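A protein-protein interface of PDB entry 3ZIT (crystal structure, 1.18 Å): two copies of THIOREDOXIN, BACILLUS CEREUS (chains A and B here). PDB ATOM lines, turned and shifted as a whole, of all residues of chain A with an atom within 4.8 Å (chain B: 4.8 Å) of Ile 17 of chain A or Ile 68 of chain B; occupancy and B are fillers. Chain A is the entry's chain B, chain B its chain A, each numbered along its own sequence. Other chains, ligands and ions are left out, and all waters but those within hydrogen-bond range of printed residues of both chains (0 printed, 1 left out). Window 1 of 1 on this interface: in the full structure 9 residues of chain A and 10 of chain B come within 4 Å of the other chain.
Ile 17 of chain A touches just these residues of chain B: Ile 17 (3.7 Å), Glu 20 (3.9 Å), Phe 21 (3.6 Å) and Ile 68 (3.8 Å).
Of the printed residues of chain A, Ile 68 of chain B touches Ile 17 and Phe 66.
Of the printed residues of chain A, Ile 17 of chain B touches Ile 17, Glu 20 and Phe 21.
Of the printed residues of chain A, Gln 72 of chain B touches Phe 66.
Of the printed residues of chain A, Glu 20 of chain B touches Ile 17.
Printed residues of chain A within 4 Å of Glu 69 of chain B: Ile 68.
Printed residues of chain B within 4 Å of Phe 66 of chain A: Phe 21, Ile 68 and Gln 72.
Val 18 of chain A touches none of the printed residues of chain B.
The nearest printed residue of chain B that does not touch Ile 17 of chain A is Phe 66 of chain B (6.2 Å).
The nearest residue of chain A that does not touch Ile 68 of chain B is Ile 68 of chain A (4.3 Å).
Hydrophobic or aromatic side chains of chain A within 4 Å of the printed part of chain B: Ile 17, Phe 21 and Phe 66.
Printed residues of chain B that touch a printed residue of chain A: Ile 17, Glu 20, Phe 21, Phe 66, Ile 68, Glu 69 and Gln 72.
Hydrophobic or aromatic side chains of chain B within 4 Å of the printed part of chain A: Ile 17, Phe 21, Phe 66 and Ile 68.
Ile 17 of chain A touches Glu 20 of chain B, and with the chains exchanged Glu 20 of chain A touches Ile 17 of chain B.
Ile 17 of chain A touches Ile 68 of chain B, but with the chains exchanged Ile 68 of chain A does not touch Ile 17 of chain B (7.1 Å).
Phe 21 of chain A touches Phe 66 of chain B, and with the chains exchanged Phe 66 of chain A touches Phe 21 of chain B.
Phe 66 of chain A touches Ile 68 of chain B, but with the chains exchanged Ile 68 of chain A does not touch Phe 66 of chain B (6.8 Å).
Positions printed for both chains: 17, 20, 21, 66 and 68.
Of the 11 pairs that touch across the chains among the printed residues, 7 have their exchanged pair printed and touching as well.
Ile 17 of chain A touches Ile 17 of chain B (CG2 to CG2, 3.7 Å).
Ile 17 of chain A touches Glu 20 of chain B.
Ile 17 of chain A touches Phe 21 of chain B.
Ile 17 of chain A touches Ile 68 of chain B.
Ile 17 of chain B touches Glu 20 of chain A.
CD1 of Phe 21 of chain A touches CE2 of Phe 66 of chain B, at 3.9 Å.
Phe 66 of chain A touches Phe 21 of chain B (CE2 to CE1, 3.96 Å).
Phe 66 of chain A touches Ile 68 of chain B (CZ to CG2, 3.9 Å).
Gln 72 of chain B touches Phe 66 of chain A (OE1 to CE2, 3.2 Å).
Glu 69 of chain B touches Ile 68 of chain A (OE2 to N, 3.7 Å).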
ATOM      1  N   PRO A  13      15.679 -31.090   2.890  1.00  0.00           N
ATOM      2  CA  PRO A  13      16.497 -29.867   2.657  1.00  0.00           C
ATOM      3  C   PRO A  13      17.478 -29.538   3.803  1.00  0.00           C
ATOM      4  O   PRO A  13      18.615 -29.137   3.529  1.00  0.00           O
ATOM      5  CB  PRO A  13      15.482 -28.748   2.429  1.00  0.00           C
ATOM      6  CG  PRO A  13      14.342 -29.453   1.812  1.00  0.00           C
ATOM      7  CD  PRO A  13      14.291 -30.818   2.572  1.00  0.00           C
ATOM      8  N   PRO A  14      17.110 -29.757   5.095  1.00  0.00           N
ATOM      9  CA  PRO A  14      18.099 -29.467   6.131  1.00  0.00           C
ATOM     10  C   PRO A  14      19.333 -30.354   6.014  1.00  0.00           C
ATOM     11  O   PRO A  14      20.440 -29.947   6.315  1.00  0.00           O
ATOM     12  CB  PRO A  14      17.313 -29.717   7.442  1.00  0.00           C
ATOM     13  CG  PRO A  14      15.843 -29.469   7.002  1.00  0.00           C
ATOM     14  CD  PRO A  14      15.771 -30.035   5.688  1.00  0.00           C
ATOM     15  N   CYS A  15      19.125 -31.618   5.562  1.00  0.00           N
ATOM     16  CA  CYS A  15      20.268 -32.488   5.300  1.00  0.00           C
ATOM     17  C   CYS A  15      21.165 -31.976   4.201  1.00  0.00           C
ATOM     18  O   CYS A  15      22.381 -32.029   4.320  1.00  0.00           O
ATOM     19  CB  CYS A  15      19.762 -33.869   4.804  1.00  0.00           C
ATOM     20  SG  CYS A  15      18.708 -34.839   5.945  1.00  0.00           S
ATOM     21  N   VAL A  16      20.554 -31.458   3.166  1.00  0.00           N
ATOM     22  CA  VAL A  16      21.334 -30.887   2.049  1.00  0.00           C
ATOM     23  C   VAL A  16      22.117 -29.677   2.532  1.00  0.00           C
ATOM     24  O   VAL A  16      23.293 -29.558   2.159  1.00  0.00           O
ATOM     25  CB  VAL A  16      20.400 -30.441   0.889  1.00  0.00           C
ATOM     26  CG1 VAL A  16      21.177 -29.620  -0.151  1.00  0.00           C
ATOM     27  CG2 VAL A  16      19.796 -31.648   0.272  1.00  0.00           C
ATOM     28  N   ILE A  17      21.483 -28.820   3.313  1.00  0.00           N
ATOM     29  CA  ILE A  17      22.152 -27.655   3.866  1.00  0.00           C
ATOM     30  C   ILE A  17      23.336 -28.073   4.711  1.00  0.00           C
ATOM     31  O   ILE A  17      24.427 -27.534   4.588  1.00  0.00           O
ATOM     32  CB  ILE A  17      21.194 -26.727   4.584  1.00  0.00           C
ATOM     33  CG1 ILE A  17      20.133 -26.240   3.607  1.00  0.00           C
ATOM     34  CG2 ILE A  17      21.969 -25.665   5.387  1.00  0.00           C
ATOM     35  CD1 ILE A  17      18.933 -25.692   4.306  1.00  0.00           C
ATOM     36  N   VAL A  18      23.157 -29.061   5.580  1.00  0.00           N
ATOM     37  CA  VAL A  18      24.268 -29.528   6.392  1.00  0.00           C
ATOM     38  C   VAL A  18      25.381 -30.084   5.549  1.00  0.00           C
ATOM     39  O   VAL A  18      26.547 -29.750   5.743  1.00  0.00           O
ATOM     40  CB  VAL A  18      23.749 -30.562   7.443  1.00  0.00           C
ATOM     41  CG1 VAL A  18      24.950 -31.343   8.065  1.00  0.00           C
ATOM     42  CG2 VAL A  18      23.008 -29.809   8.509  1.00  0.00           C
ATOM     43  N   LYS A  19      25.057 -30.959   4.576  1.00  0.00           N
ATOM     44  CA  LYS A  19      26.122 -31.523   3.746  1.00  0.00           C
ATOM     45  C   LYS A  19      26.852 -30.429   2.965  1.00  0.00           C
ATOM     46  O   LYS A  19      28.072 -30.452   2.879  1.00  0.00           O
ATOM     47  CB  LYS A  19      25.543 -32.556   2.802  1.00  0.00           C
ATOM     48  CG  LYS A  19      25.135 -33.860   3.420  1.00  0.00           C
ATOM     49  CD  LYS A  19      24.261 -34.716   2.445  1.00  0.00           C
ATOM     50  CE  LYS A  19      23.872 -36.095   2.647  1.00  0.00           C
ATOM     51  NZ  LYS A  19      23.375 -36.352   1.259  1.00  0.00           N
ATOM     52  N   GLU A  20      26.125 -29.468   2.399  1.00  0.00           N
ATOM     53  CA  GLU A  20      26.780 -28.407   1.659  1.00  0.00           C
ATOM     54  C   GLU A  20      27.624 -27.541   2.519  1.00  0.00           C
ATOM     55  O   GLU A  20      28.688 -27.067   2.082  1.00  0.00           O
ATOM     56  CB  GLU A  20      25.760 -27.646   0.821  1.00  0.00           C
ATOM     57  CG  GLU A  20      25.111 -28.566  -0.274  1.00  0.00           C
ATOM     58  CD  GLU A  20      26.138 -29.097  -1.320  1.00  0.00           C
ATOM     59  OE1 GLU A  20      26.963 -28.268  -1.728  1.00  0.00           O
ATOM     60  OE2 GLU A  20      26.106 -30.308  -1.755  1.00  0.00           O
ATOM     61  N   PHE A  21      27.159 -27.255   3.746  1.00  0.00           N
ATOM     62  CA  PHE A  21      27.957 -26.542   4.753  1.00  0.00           C
ATOM     63  C   PHE A  21      29.306 -27.324   4.995  1.00  0.00           C
ATOM     64  O   PHE A  21      30.360 -26.734   5.046  1.00  0.00           O
ATOM     65  CB  PHE A  21      27.130 -26.361   5.989  1.00  0.00           C
ATOM     66  CG  PHE A  21      27.916 -25.830   7.167  1.00  0.00           C
ATOM     67  CD1 PHE A  21      28.153 -24.428   7.219  1.00  0.00           C
ATOM     68  CD2 PHE A  21      28.416 -26.642   8.129  1.00  0.00           C
ATOM     69  CE1 PHE A  21      28.890 -23.833   8.215  1.00  0.00           C
ATOM     70  CE2 PHE A  21      29.204 -26.076   9.214  1.00  0.00           C
ATOM     71  CZ  PHE A  21      29.356 -24.653   9.184  1.00  0.00           C
ATOM     72  N   PHE A  66      19.040 -29.752  13.046  1.00  0.00           N
ATOM     73  CA  PHE A  66      19.728 -28.639  12.341  1.00  0.00           C
ATOM     74  C   PHE A  66      20.378 -27.721  13.330  1.00  0.00           C
ATOM     75  O   PHE A  66      19.708 -26.890  13.871  1.00  0.00           O
ATOM     76  CB  PHE A  66      18.716 -27.923  11.453  1.00  0.00           C
ATOM     77  CG  PHE A  66      19.289 -26.959  10.513  1.00  0.00           C
ATOM     78  CD1 PHE A  66      19.953 -27.441   9.420  1.00  0.00           C
ATOM     79  CD2 PHE A  66      19.275 -25.572  10.726  1.00  0.00           C
ATOM     80  CE1 PHE A  66      20.512 -26.574   8.457  1.00  0.00           C
ATOM     81  CE2 PHE A  66      19.857 -24.668   9.831  1.00  0.00           C
ATOM     82  CZ  PHE A  66      20.437 -25.192   8.688  1.00  0.00           C
ATOM     83  N   ILE A  68      23.689 -25.699  13.211  1.00  0.00           N
ATOM     84  CA  ILE A  68      24.919 -25.320  12.465  1.00  0.00           C
ATOM     85  C   ILE A  68      26.026 -24.821  13.390  1.00  0.00           C
ATOM     86  O   ILE A  68      27.189 -25.184  13.219  1.00  0.00           O
ATOM     87  CB  ILE A  68      24.591 -24.267  11.405  1.00  0.00           C
ATOM     88  CG1 ILE A  68      23.621 -24.797  10.360  1.00  0.00           C
ATOM     89  CG2 ILE A  68      25.867 -23.746  10.756  1.00  0.00           C
ATOM     90  CD1 ILE A  68      24.103 -26.057   9.583  1.00  0.00           C
ATOM     91  N   ILE B  17      23.513 -22.223  -0.478  1.00  0.00           N
ATOM     92  CA  ILE B  17      23.070 -22.763   0.758  1.00  0.00           C
ATOM     93  C   ILE B  17      22.019 -21.836   1.426  1.00  0.00           C
ATOM     94  O   ILE B  17      21.004 -22.285   1.959  1.00  0.00           O
ATOM     95  CB  ILE B  17      24.258 -23.043   1.642  1.00  0.00           C
ATOM     96  CG1 ILE B  17      25.224 -24.011   0.947  1.00  0.00           C
ATOM     97  CG2 ILE B  17      23.729 -23.546   2.979  1.00  0.00           C
ATOM     98  CD1 ILE B  17      26.556 -24.157   1.728  1.00  0.00           C
ATOM     99  N   GLU B  20      18.747 -22.144  -0.177  1.00  0.00           N
ATOM    100  CA  GLU B  20      18.022 -23.374   0.190  1.00  0.00           C
ATOM    101  C   GLU B  20      17.422 -23.281   1.606  1.00  0.00           C
ATOM    102  O   GLU B  20      16.318 -23.809   1.835  1.00  0.00           O
ATOM    103  CB  GLU B  20      18.998 -24.533   0.014  1.00  0.00           C
ATOM    104  CG  GLU B  20      19.386 -24.634  -1.500  1.00  0.00           C
ATOM    105  CD  GLU B  20      18.163 -24.677  -2.461  1.00  0.00           C
ATOM    106  OE1 GLU B  20      17.258 -25.529  -2.263  1.00  0.00           O
ATOM    107  OE2 GLU B  20      18.076 -23.899  -3.432  1.00  0.00           O
ATOM    108  N   PHE B  21      18.101 -22.639   2.500  1.00  0.00           N
ATOM    109  CA  PHE B  21      17.567 -22.425   3.817  1.00  0.00           C
ATOM    110  C   PHE B  21      16.289 -21.556   3.738  1.00  0.00           C
ATOM    111  O   PHE B  21      15.260 -21.902   4.377  1.00  0.00           O
ATOM    112  CB  PHE B  21      18.592 -21.765   4.657  1.00  0.00           C
ATOM    113  CG  PHE B  21      18.085 -21.346   6.014  1.00  0.00           C
ATOM    114  CD1 PHE B  21      17.945 -22.312   7.020  1.00  0.00           C
ATOM    115  CD2 PHE B  21      17.669 -20.059   6.264  1.00  0.00           C
ATOM    116  CE1 PHE B  21      17.441 -21.963   8.251  1.00  0.00           C
ATOM    117  CE2 PHE B  21      17.197 -19.686   7.488  1.00  0.00           C
ATOM    118  CZ  PHE B  21      17.052 -20.644   8.489  1.00  0.00           C
ATOM    119  N   PHE B  66      28.220 -15.509   5.028  1.00  0.00           N
ATOM    120  CA  PHE B  66      27.600 -16.807   5.204  1.00  0.00           C
ATOM    121  C   PHE B  66      27.295 -17.021   6.684  1.00  0.00           C
ATOM    122  O   PHE B  66      28.164 -17.452   7.468  1.00  0.00           O
ATOM    123  CB  PHE B  66      28.550 -17.882   4.618  1.00  0.00           C
ATOM    124  CG  PHE B  66      27.960 -19.273   4.535  1.00  0.00           C
ATOM    125  CD1 PHE B  66      26.587 -19.494   4.322  1.00  0.00           C
ATOM    126  CD2 PHE B  66      28.830 -20.370   4.614  1.00  0.00           C
ATOM    127  CE1 PHE B  66      26.075 -20.798   4.258  1.00  0.00           C
ATOM    128  CE2 PHE B  66      28.331 -21.675   4.508  1.00  0.00           C
ATOM    129  CZ  PHE B  66      26.939 -21.870   4.344  1.00  0.00           C
ATOM    130  N   GLN B  67      26.077 -16.735   7.123  1.00  0.00           N
ATOM    131  CA  GLN B  67      25.779 -16.816   8.508  1.00  0.00           C
ATOM    132  C   GLN B  67      24.470 -17.431   8.590  1.00  0.00           C
ATOM    133  O   GLN B  67      23.531 -16.702   8.837  1.00  0.00           O
ATOM    134  CB  GLN B  67      25.594 -15.482   9.156  1.00  0.00           C
ATOM    135  CG  GLN B  67      26.732 -14.510   9.175  1.00  0.00           C
ATOM    136  CD  GLN B  67      26.286 -13.285   9.974  1.00  0.00           C
ATOM    137  OE1 GLN B  67      25.712 -13.415  11.075  1.00  0.00           O
ATOM    138  NE2 GLN B  67      26.490 -12.110   9.414  1.00  0.00           N
ATOM    139  N   ILE B  68      24.327 -18.751   8.354  1.00  0.00           N
ATOM    140  CA  ILE B  68      22.936 -19.331   8.411  1.00  0.00           C
ATOM    141  C   ILE B  68      22.167 -19.093   9.723  1.00  0.00           C
ATOM    142  O   ILE B  68      20.928 -18.928   9.652  1.00  0.00           O
ATOM    143  CB  ILE B  68      22.897 -20.861   8.138  1.00  0.00           C
ATOM    144  CG1 ILE B  68      23.451 -21.128   6.780  1.00  0.00           C
ATOM    145  CG2 ILE B  68      21.480 -21.424   8.212  1.00  0.00           C
ATOM    146  CD1 ILE B  68      23.787 -22.611   6.606  1.00  0.00           C
ATOM    147  N   GLU B  69      22.817 -19.039  10.887  1.00  0.00           N
ATOM    148  CA  GLU B  69      22.056 -18.939  12.165  1.00  0.00           C
ATOM    149  C   GLU B  69      21.348 -17.611  12.328  1.00  0.00           C
ATOM    150  O   GLU B  69      20.240 -17.587  12.899  1.00  0.00           O
ATOM    151  CB  GLU B  69      22.849 -19.426  13.424  1.00  0.00           C
ATOM    152  CG  GLU B  69      22.246 -20.776  13.936  1.00  0.00           C
ATOM    153  CD  GLU B  69      22.845 -21.423  15.225  1.00  0.00           C
ATOM    154  OE1 GLU B  69      23.062 -20.650  16.245  1.00  0.00           O
ATOM    155  OE2 GLU B  69      23.048 -22.712  15.227  1.00  0.00           O
ATOM    156  N   LYS B  70      21.896 -16.527  11.746  1.00  0.00           N
ATOM    157  CA  LYS B  70      21.183 -15.232  11.883  1.00  0.00           C
ATOM    158  C   LYS B  70      19.914 -15.166  11.047  1.00  0.00           C
ATOM    159  O   LYS B  70      18.938 -14.494  11.457  1.00  0.00           O
ATOM    160  CB  LYS B  70      22.077 -14.020  11.630  1.00  0.00           C
ATOM    161  CG  LYS B  70      23.224 -13.856  12.599  1.00  0.00           C
ATOM    162  CD  LYS B  70      23.487 -12.376  12.855  1.00  0.00           C
ATOM    163  CE  LYS B  70      24.664 -12.209  13.802  1.00  0.00           C
ATOM    164  NZ  LYS B  70      25.446 -10.946  13.582  1.00  0.00           N
ATOM    165  N   LEU B  71      19.911 -15.852   9.901  1.00  0.00           N
ATOM    166  CA  LEU B  71      18.661 -15.881   9.148  1.00  0.00           C
ATOM    167  C   LEU B  71      17.568 -16.438  10.115  1.00  0.00           C
ATOM    168  O   LEU B  71      16.513 -15.804  10.339  1.00  0.00           O
ATOM    169  CB  LEU B  71      18.806 -16.635   7.814  1.00  0.00           C
ATOM    170  CG  LEU B  71      19.936 -15.999   7.035  1.00  0.00           C
ATOM    171  CD1 LEU B  71      20.128 -16.824   5.746  1.00  0.00           C
ATOM    172  CD2 LEU B  71      19.774 -14.499   6.786  1.00  0.00           C
ATOM    173  N   GLN B  72      17.855 -17.559  10.785  1.00  0.00           N
ATOM    174  CA  GLN B  72      16.935 -18.070  11.842  1.00  0.00           C
ATOM    175  C   GLN B  72      16.518 -17.014  12.906  1.00  0.00           C
ATOM    176  O   GLN B  72      15.327 -16.842  13.190  1.00  0.00           O
ATOM    177  CB  GLN B  72      17.536 -19.279  12.557  1.00  0.00           C
ATOM    178  CG  GLN B  72      18.170 -20.333  11.667  1.00  0.00           C
ATOM    179  CD  GLN B  72      18.909 -21.428  12.441  1.00  0.00           C
ATOM    180  OE1 GLN B  72      19.639 -22.245  11.863  1.00  0.00           O
ATOM    181  NE2 GLN B  72      18.754 -21.431  13.736  1.00  0.00           N
